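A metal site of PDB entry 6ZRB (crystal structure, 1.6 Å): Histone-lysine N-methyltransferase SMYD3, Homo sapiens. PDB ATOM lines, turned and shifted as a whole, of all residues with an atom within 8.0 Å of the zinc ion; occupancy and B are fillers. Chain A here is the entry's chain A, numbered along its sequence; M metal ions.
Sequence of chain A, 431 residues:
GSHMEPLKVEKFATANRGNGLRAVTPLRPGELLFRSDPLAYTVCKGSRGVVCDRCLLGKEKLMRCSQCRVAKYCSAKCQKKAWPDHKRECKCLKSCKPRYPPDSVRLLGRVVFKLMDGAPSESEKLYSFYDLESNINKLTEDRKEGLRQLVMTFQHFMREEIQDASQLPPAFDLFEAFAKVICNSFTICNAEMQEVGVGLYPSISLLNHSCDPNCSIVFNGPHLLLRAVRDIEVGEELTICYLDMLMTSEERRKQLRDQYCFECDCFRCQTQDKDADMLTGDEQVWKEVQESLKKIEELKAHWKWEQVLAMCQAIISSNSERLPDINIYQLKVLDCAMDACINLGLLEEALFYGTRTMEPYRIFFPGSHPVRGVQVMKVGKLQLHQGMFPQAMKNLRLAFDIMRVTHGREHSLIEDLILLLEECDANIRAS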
ATOM      1  N   ASP A  53      11.299 -29.216   8.660  1.00  0.00           N
ATOM      2  CA  ASP A  53       9.978 -28.725   8.173  1.00  0.00           C
ATOM      3  C   ASP A  53       9.521 -29.474   6.915  1.00  0.00           C
ATOM      4  O   ASP A  53       8.319 -29.665   6.754  1.00  0.00           O
ATOM      5  CB  ASP A  53      10.050 -27.238   7.809  1.00  0.00           C
ATOM      6  CG  ASP A  53       9.599 -26.285   8.900  1.00  0.00           C
ATOM      7  OD1 ASP A  53      10.050 -26.425  10.071  1.00  0.00           O
ATOM      8  OD2 ASP A  53       8.801 -25.401   8.577  1.00  0.00           O
ATOM      9  N   ARG A  64      18.168 -22.996  10.125  1.00  0.00           N
ATOM     10  CA  ARG A  64      16.912 -22.208  10.179  1.00  0.00           C
ATOM     11  C   ARG A  64      16.837 -21.279   8.979  1.00  0.00           C
ATOM     12  O   ARG A  64      17.877 -20.799   8.476  1.00  0.00           O
ATOM     13  CB  ARG A  64      16.772 -21.460  11.497  1.00  0.00           C
ATOM     14  CG  ARG A  64      17.751 -20.318  11.669  1.00  0.00           C
ATOM     15  CD  ARG A  64      17.720 -19.779  13.086  1.00  0.00           C
ATOM     16  NE  ARG A  64      18.895 -18.929  13.289  1.00  0.00           N
ATOM     17  CZ  ARG A  64      19.119 -18.242  14.385  1.00  0.00           C
ATOM     18  NH1 ARG A  64      20.211 -17.515  14.489  1.00  0.00           N
ATOM     19  NH2 ARG A  64      18.250 -18.282  15.376  1.00  0.00           N
ATOM     20  N   CYS A  65      15.608 -21.030   8.514  1.00  0.00           N
ATOM     21  CA  CYS A  65      15.288 -19.924   7.597  1.00  0.00           C
ATOM     22  C   CYS A  65      15.777 -18.616   8.216  1.00  0.00           C
ATOM     23  O   CYS A  65      15.369 -18.263   9.339  1.00  0.00           O
ATOM     24  CB  CYS A  65      13.800 -19.829   7.342  1.00  0.00           C
ATOM     25  SG  CYS A  65      13.392 -18.477   6.211  1.00  0.00           S
ATOM     26  N   SER A  66      16.658 -17.903   7.528  1.00  0.00           N
ATOM     27  CA  SER A  66      17.224 -16.668   8.088  1.00  0.00           C
ATOM     28  C   SER A  66      16.139 -15.606   8.267  1.00  0.00           C
ATOM     29  O   SER A  66      16.254 -14.821   9.227  1.00  0.00           O
ATOM     30  CB  SER A  66      18.343 -16.168   7.242  1.00  0.00           C
ATOM     31  OG  SER A  66      18.855 -15.014   7.870  1.00  0.00           O
ATOM     32  N   GLN A  67      15.147 -15.565   7.371  1.00  0.00           N
ATOM     33  CA  GLN A  67      14.123 -14.482   7.339  1.00  0.00           C
ATOM     34  C   GLN A  67      13.220 -14.631   8.564  1.00  0.00           C
ATOM     35  O   GLN A  67      13.096 -13.675   9.344  1.00  0.00           O
ATOM     36  CB  GLN A  67      13.372 -14.464   6.011  1.00  0.00           C
ATOM     37  CG  GLN A  67      12.367 -13.319   5.942  1.00  0.00           C
ATOM     38  CD  GLN A  67      11.888 -12.973   4.544  1.00  0.00           C
ATOM     39  OE1 GLN A  67      12.189 -11.905   4.016  1.00  0.00           O
ATOM     40  NE2 GLN A  67      11.095 -13.861   3.956  1.00  0.00           N
ATOM     41  N   CYS A  68      12.621 -15.810   8.792  1.00  0.00           N
ATOM     42  CA  CYS A  68      11.651 -15.977   9.906  1.00  0.00           C
ATOM     43  C   CYS A  68      12.308 -16.589  11.140  1.00  0.00           C
ATOM     44  O   CYS A  68      11.794 -16.345  12.242  1.00  0.00           O
ATOM     45  CB  CYS A  68      10.424 -16.785   9.485  1.00  0.00           C
ATOM     46  SG  CYS A  68      10.793 -18.487   8.972  1.00  0.00           S
ATOM     47  N   ARG A  69      13.323 -17.440  10.973  1.00  0.00           N
ATOM     48  CA  ARG A  69      13.979 -18.213  12.055  1.00  0.00           C
ATOM     49  C   ARG A  69      12.997 -19.143  12.764  1.00  0.00           C
ATOM     50  O   ARG A  69      13.304 -19.573  13.904  1.00  0.00           O
ATOM     51  CB  ARG A  69      14.657 -17.256  13.044  1.00  0.00           C
ATOM     52  CG  ARG A  69      15.880 -16.599  12.435  1.00  0.00           C
ATOM     53  CD  ARG A  69      16.568 -15.692  13.411  1.00  0.00           C
ATOM     54  NE  ARG A  69      17.884 -15.323  12.920  1.00  0.00           N
ATOM     55  CZ  ARG A  69      18.740 -14.576  13.608  1.00  0.00           C
ATOM     56  NH1 ARG A  69      19.927 -14.295  13.103  1.00  0.00           N
ATOM     57  NH2 ARG A  69      18.410 -14.165  14.827  1.00  0.00           N
ATOM     58  N   VAL A  70      11.906 -19.518  12.085  1.00  0.00           N
ATOM     59  CA  VAL A  70      10.895 -20.478  12.605  1.00  0.00           C
ATOM     60  C   VAL A  70      11.014 -21.780  11.806  1.00  0.00           C
ATOM     61  O   VAL A  70      11.114 -22.861  12.440  1.00  0.00           O
ATOM     62  CB  VAL A  70       9.491 -19.864  12.534  1.00  0.00           C
ATOM     63  CG1 VAL A  70       8.406 -20.886  12.828  1.00  0.00           C
ATOM     64  CG2 VAL A  70       9.354 -18.657  13.455  1.00  0.00           C
ATOM     65  N   ALA A  71      10.996 -21.705  10.476  1.00  0.00           N
ATOM     66  CA  ALA A  71      11.166 -22.896   9.615  1.00  0.00           C
ATOM     67  C   ALA A  71      12.596 -23.403   9.795  1.00  0.00           C
ATOM     68  O   ALA A  71      13.531 -22.575   9.751  1.00  0.00           O
ATOM     69  CB  ALA A  71      10.875 -22.587   8.168  1.00  0.00           C
ATOM     70  N   LYS A  72      12.772 -24.697   9.984  1.00  0.00           N
ATOM     71  CA  LYS A  72      14.110 -25.310  10.153  1.00  0.00           C
ATOM     72  C   LYS A  72      14.191 -26.557   9.295  1.00  0.00           C
ATOM     73  O   LYS A  72      13.161 -27.228   9.086  1.00  0.00           O
ATOM     74  CB  LYS A  72      14.391 -25.595  11.627  1.00  0.00           C
ATOM     75  CG  LYS A  72      14.423 -24.329  12.477  1.00  0.00           C
ATOM     76  CD  LYS A  72      15.022 -24.530  13.831  1.00  0.00           C
ATOM     77  CE  LYS A  72      14.920 -23.292  14.690  1.00  0.00           C
ATOM     78  NZ  LYS A  72      15.368 -23.586  16.070  1.00  0.00           N
ATOM     79  N   TYR A  73      15.399 -26.856   8.819  1.00  0.00           N
ATOM     80  CA  TYR A  73      15.598 -27.863   7.755  1.00  0.00           C
ATOM     81  C   TYR A  73      16.827 -28.715   8.070  1.00  0.00           C
ATOM     82  O   TYR A  73      17.750 -28.256   8.764  1.00  0.00           O
ATOM     83  CB  TYR A  73      15.734 -27.175   6.400  1.00  0.00           C
ATOM     84  CG  TYR A  73      14.561 -26.281   6.052  1.00  0.00           C
ATOM     85  CD1 TYR A  73      13.397 -26.819   5.530  1.00  0.00           C
ATOM     86  CD2 TYR A  73      14.596 -24.910   6.285  1.00  0.00           C
ATOM     87  CE1 TYR A  73      12.307 -26.024   5.207  1.00  0.00           C
ATOM     88  CE2 TYR A  73      13.519 -24.101   5.950  1.00  0.00           C
ATOM     89  CZ  TYR A  73      12.364 -24.661   5.421  1.00  0.00           C
ATOM     90  OH  TYR A  73      11.289 -23.867   5.079  1.00  0.00           O
ATOM     91  N   GLN A  79      15.665 -26.972   2.585  1.00  0.00           N
ATOM     92  CA  GLN A  79      15.349 -25.521   2.766  1.00  0.00           C
ATOM     93  C   GLN A  79      14.973 -24.929   1.404  1.00  0.00           C
ATOM     94  O   GLN A  79      13.981 -24.201   1.303  1.00  0.00           O
ATOM     95  CB  GLN A  79      16.518 -24.789   3.416  1.00  0.00           C
ATOM     96  CG  GLN A  79      16.214 -23.318   3.636  1.00  0.00           C
ATOM     97  CD  GLN A  79      17.207 -22.598   4.513  1.00  0.00           C
ATOM     98  OE1 GLN A  79      18.057 -23.219   5.160  1.00  0.00           O
ATOM     99  NE2 GLN A  79      17.066 -21.286   4.575  1.00  0.00           N
ATOM    100  N   TRP A  83      11.077 -23.679  -0.220  1.00  0.00           N
ATOM    101  CA  TRP A  83      10.929 -22.198  -0.289  1.00  0.00           C
ATOM    102  C   TRP A  83       9.620 -21.814  -0.964  1.00  0.00           C
ATOM    103  O   TRP A  83       8.873 -21.008  -0.410  1.00  0.00           O
ATOM    104  CB  TRP A  83      12.146 -21.541  -0.948  1.00  0.00           C
ATOM    105  CG  TRP A  83      11.952 -20.066  -1.108  1.00  0.00           C
ATOM    106  CD1 TRP A  83      11.807 -19.381  -2.282  1.00  0.00           C
ATOM    107  CD2 TRP A  83      11.812 -19.100  -0.058  1.00  0.00           C
ATOM    108  NE1 TRP A  83      11.624 -18.056  -2.031  1.00  0.00           N
ATOM    109  CE2 TRP A  83      11.630 -17.838  -0.686  1.00  0.00           C
ATOM    110  CE3 TRP A  83      11.862 -19.145   1.330  1.00  0.00           C
ATOM    111  CZ2 TRP A  83      11.472 -16.668   0.047  1.00  0.00           C
ATOM    112  CZ3 TRP A  83      11.705 -17.990   2.055  1.00  0.00           C
ATOM    113  CH2 TRP A  83      11.525 -16.757   1.420  1.00  0.00           C
ATOM    114  N   HIS A  86       6.855 -22.084   1.439  1.00  0.00           N
ATOM    115  CA  HIS A  86       7.151 -21.366   2.705  1.00  0.00           C
ATOM    116  C   HIS A  86       7.181 -19.839   2.506  1.00  0.00           C
ATOM    117  O   HIS A  86       7.044 -19.123   3.495  1.00  0.00           O
ATOM    118  CB  HIS A  86       8.484 -21.872   3.295  1.00  0.00           C
ATOM    119  CG  HIS A  86       8.956 -21.104   4.470  1.00  0.00           C
ATOM    120  ND1 HIS A  86       8.270 -21.076   5.642  1.00  0.00           N
ATOM    121  CD2 HIS A  86      10.043 -20.312   4.647  1.00  0.00           C
ATOM    122  CE1 HIS A  86       8.876 -20.280   6.506  1.00  0.00           C
ATOM    123  NE2 HIS A  86       9.977 -19.821   5.917  1.00  0.00           N
ATOM    124  N   LYS A  87       7.363 -19.370   1.269  1.00  0.00           N
ATOM    125  CA  LYS A  87       7.679 -17.950   0.941  1.00  0.00           C
ATOM    126  C   LYS A  87       6.680 -17.003   1.601  1.00  0.00           C
ATOM    127  O   LYS A  87       7.111 -16.028   2.257  1.00  0.00           O
ATOM    128  CB  LYS A  87       7.671 -17.832  -0.574  1.00  0.00           C
ATOM    129  CG  LYS A  87       7.864 -16.459  -1.182  1.00  0.00           C
ATOM    130  CD  LYS A  87       7.710 -16.494  -2.705  1.00  0.00           C
ATOM    131  CE  LYS A  87       8.172 -17.816  -3.319  1.00  0.00           C
ATOM    132  NZ  LYS A  87       8.060 -17.858  -4.799  1.00  0.00           N
ATOM    133  N   ARG A  88       5.375 -17.252   1.423  1.00  0.00           N
ATOM    134  CA  ARG A  88       4.339 -16.313   1.911  1.00  0.00           C
ATOM    135  C   ARG A  88       4.151 -16.472   3.424  1.00  0.00           C
ATOM    136  O   ARG A  88       3.982 -15.444   4.104  1.00  0.00           O
ATOM    137  CB  ARG A  88       3.030 -16.464   1.127  1.00  0.00           C
ATOM    138  CG  ARG A  88       3.195 -16.175  -0.362  1.00  0.00           C
ATOM    139  CD  ARG A  88       1.886 -16.108  -1.111  1.00  0.00           C
ATOM    140  NE  ARG A  88       1.027 -15.036  -0.673  1.00  0.00           N
ATOM    141  CZ  ARG A  88      -0.253 -14.907  -1.045  1.00  0.00           C
ATOM    142  NH1 ARG A  88      -0.792 -15.774  -1.879  1.00  0.00           N
ATOM    143  NH2 ARG A  88      -0.981 -13.910  -0.574  1.00  0.00           N
ATOM    144  N   GLU A  89       4.198 -17.687   3.972  1.00  0.00           N
ATOM    145  CA  GLU A  89       4.040 -17.850   5.436  1.00  0.00           C
ATOM    146  C   GLU A  89       5.257 -17.236   6.142  1.00  0.00           C
ATOM    147  O   GLU A  89       5.135 -16.813   7.297  1.00  0.00           O
ATOM    148  CB  GLU A  89       3.781 -19.304   5.810  1.00  0.00           C
ATOM    149  CG  GLU A  89       4.997 -20.169   5.843  1.00  0.00           C
ATOM    150  CD  GLU A  89       4.927 -21.511   6.533  1.00  0.00           C
ATOM    151  OE1 GLU A  89       3.873 -21.894   7.074  1.00  0.00           O
ATOM    152  OE2 GLU A  89       5.942 -22.201   6.518  1.00  0.00           O
ATOM    153  N   CYS A  90       6.408 -17.205   5.474  1.00  0.00           N
ATOM    154  CA  CYS A  90       7.665 -16.728   6.087  1.00  0.00           C
ATOM    155  C   CYS A  90       7.454 -15.278   6.564  1.00  0.00           C
ATOM    156  O   CYS A  90       7.759 -15.006   7.731  1.00  0.00           O
ATOM    157  CB  CYS A  90       8.800 -16.859   5.084  1.00  0.00           C
ATOM    158  SG  CYS A  90      10.367 -16.278   5.766  1.00  0.00           S
ATOM    159  N   LYS A  91       6.894 -14.439   5.690  1.00  0.00           N
ATOM    160  CA  LYS A  91       6.570 -13.012   5.974  1.00  0.00           C
ATOM    161  C   LYS A  91       5.653 -12.948   7.204  1.00  0.00           C
ATOM    162  O   LYS A  91       5.858 -12.066   8.034  1.00  0.00           O
ATOM    163  CB  LYS A  91       5.973 -12.331   4.744  1.00  0.00           C
ATOM    164  CG  LYS A  91       6.847 -12.372   3.490  1.00  0.00           C
ATOM    165  CD  LYS A  91       6.551 -11.284   2.476  1.00  0.00           C
ATOM    166  CE  LYS A  91       6.858 -11.694   1.043  1.00  0.00           C
ATOM    167  NZ  LYS A  91       5.894 -12.694   0.502  1.00  0.00           N
ATOM    168  N   CYS A  92       4.702 -13.887   7.341  1.00  0.00           N
ATOM    169  CA  CYS A  92       3.706 -13.871   8.443  1.00  0.00           C
ATOM    170  C   CYS A  92       4.326 -14.392   9.745  1.00  0.00           C
ATOM    171  O   CYS A  92       4.020 -13.826  10.816  1.00  0.00           O
ATOM    172  CB  CYS A  92       2.478 -14.700   8.094  1.00  0.00           C
ATOM    173  SG  CYS A  92       1.685 -14.249   6.532  1.00  0.00           S
ATOM    174  N   LEU A  93       5.152 -15.439   9.705  1.00  0.00           N
ATOM    175  CA  LEU A  93       5.812 -15.990  10.912  1.00  0.00           C
ATOM    176  C   LEU A  93       6.795 -14.953  11.459  1.00  0.00           C
ATOM    177  O   LEU A  93       6.894 -14.827  12.697  1.00  0.00           O
ATOM    178  CB  LEU A  93       6.528 -17.312  10.599  1.00  0.00           C
ATOM    179  CG  LEU A  93       5.627 -18.498  10.253  1.00  0.00           C
ATOM    180  CD1 LEU A  93       6.431 -19.607   9.596  1.00  0.00           C
ATOM    181  CD2 LEU A  93       4.896 -19.030  11.479  1.00  0.00           C
ATOM    182  N   LYS A  94       7.498 -14.248  10.565  1.00  0.00           N
ATOM    183  CA  LYS A  94       8.432 -13.154  10.952  1.00  0.00           C
ATOM    184  C   LYS A  94       7.600 -12.059  11.631  1.00  0.00           C
ATOM    185  O   LYS A  94       7.822 -11.831  12.831  1.00  0.00           O
ATOM    186  CB  LYS A  94       9.189 -12.590   9.744  1.00  0.00           C
ATOM    187  CG  LYS A  94      10.225 -11.524  10.088  1.00  0.00           C
ATOM    188  CD  LYS A  94      10.672 -10.682   8.917  1.00  0.00           C
ATOM    189  CE  LYS A  94      11.893  -9.836   9.233  1.00  0.00           C
ATOM    190  NZ  LYS A  94      13.135 -10.637   9.200  1.00  0.00           N
ATOM    191  N   ARG A 106      -1.419 -22.437  11.013  1.00  0.00           N
ATOM    192  CA  ARG A 106      -0.281 -22.538  10.077  1.00  0.00           C
ATOM    193  C   ARG A 106      -0.672 -23.457   8.912  1.00  0.00           C
ATOM    194  O   ARG A 106      -0.341 -23.142   7.748  1.00  0.00           O
ATOM    195  CB  ARG A 106       0.957 -23.041  10.804  1.00  0.00           C
ATOM    196  CG  ARG A 106       2.171 -23.006   9.896  1.00  0.00           C
ATOM    197  CD  ARG A 106       3.470 -23.254  10.636  1.00  0.00           C
ATOM    198  NE  ARG A 106       4.590 -23.180   9.679  1.00  0.00           N
ATOM    199  CZ  ARG A 106       5.828 -23.588   9.952  1.00  0.00           C
ATOM    200  NH1 ARG A 106       6.122 -24.069  11.147  1.00  0.00           N
ATOM    201  NH2 ARG A 106       6.774 -23.463   9.033  1.00  0.00           N
HETATM  202 ZN    ZN M   1      11.176 -18.273   6.694  1.00  0.00          ZN
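SG of Cys 68 sits close to N of Val 70 (3.5 Å). SG of Cys 68 lies close to N of Ala 71, 3.6 Å away. A ring nitrogen (ND1) of His 86 is in hydrogen-bond range of the side-chain carboxylate (OE2) of Glu 89, at 2.7 Å. The side-chain sulfur (SG) of Cys 90 lies close to the side-chain amide nitrogen (NE2) of Gln 67 (3.1 Å). The side-chain sulfur (SG) of Cys 65 lies close to the backbone NH (N) of Gln 67, at 3.6 Å. The backbone carbonyl oxygen (O) of Ala 71 lies within hydrogen-bond range of the backbone NH (N) of Cys 65, 2.9 Å away.
Within 4 Å of the zinc ion: Cys 65, Cys 68, His 86 and Cys 90. Along chain A the residues within 4 Å of the zinc ion span positions 65 to 90. The nearest printed residue that does not touch the zinc ion is Gln 67 (4.4 Å).
The zinc ion is bound by NE2 of His 86 (2.1 Å), SG of Cys 65 (2.3 Å), SG of Cys 68 (2.3 Å) and SG of Cys 90 (2.3 Å).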
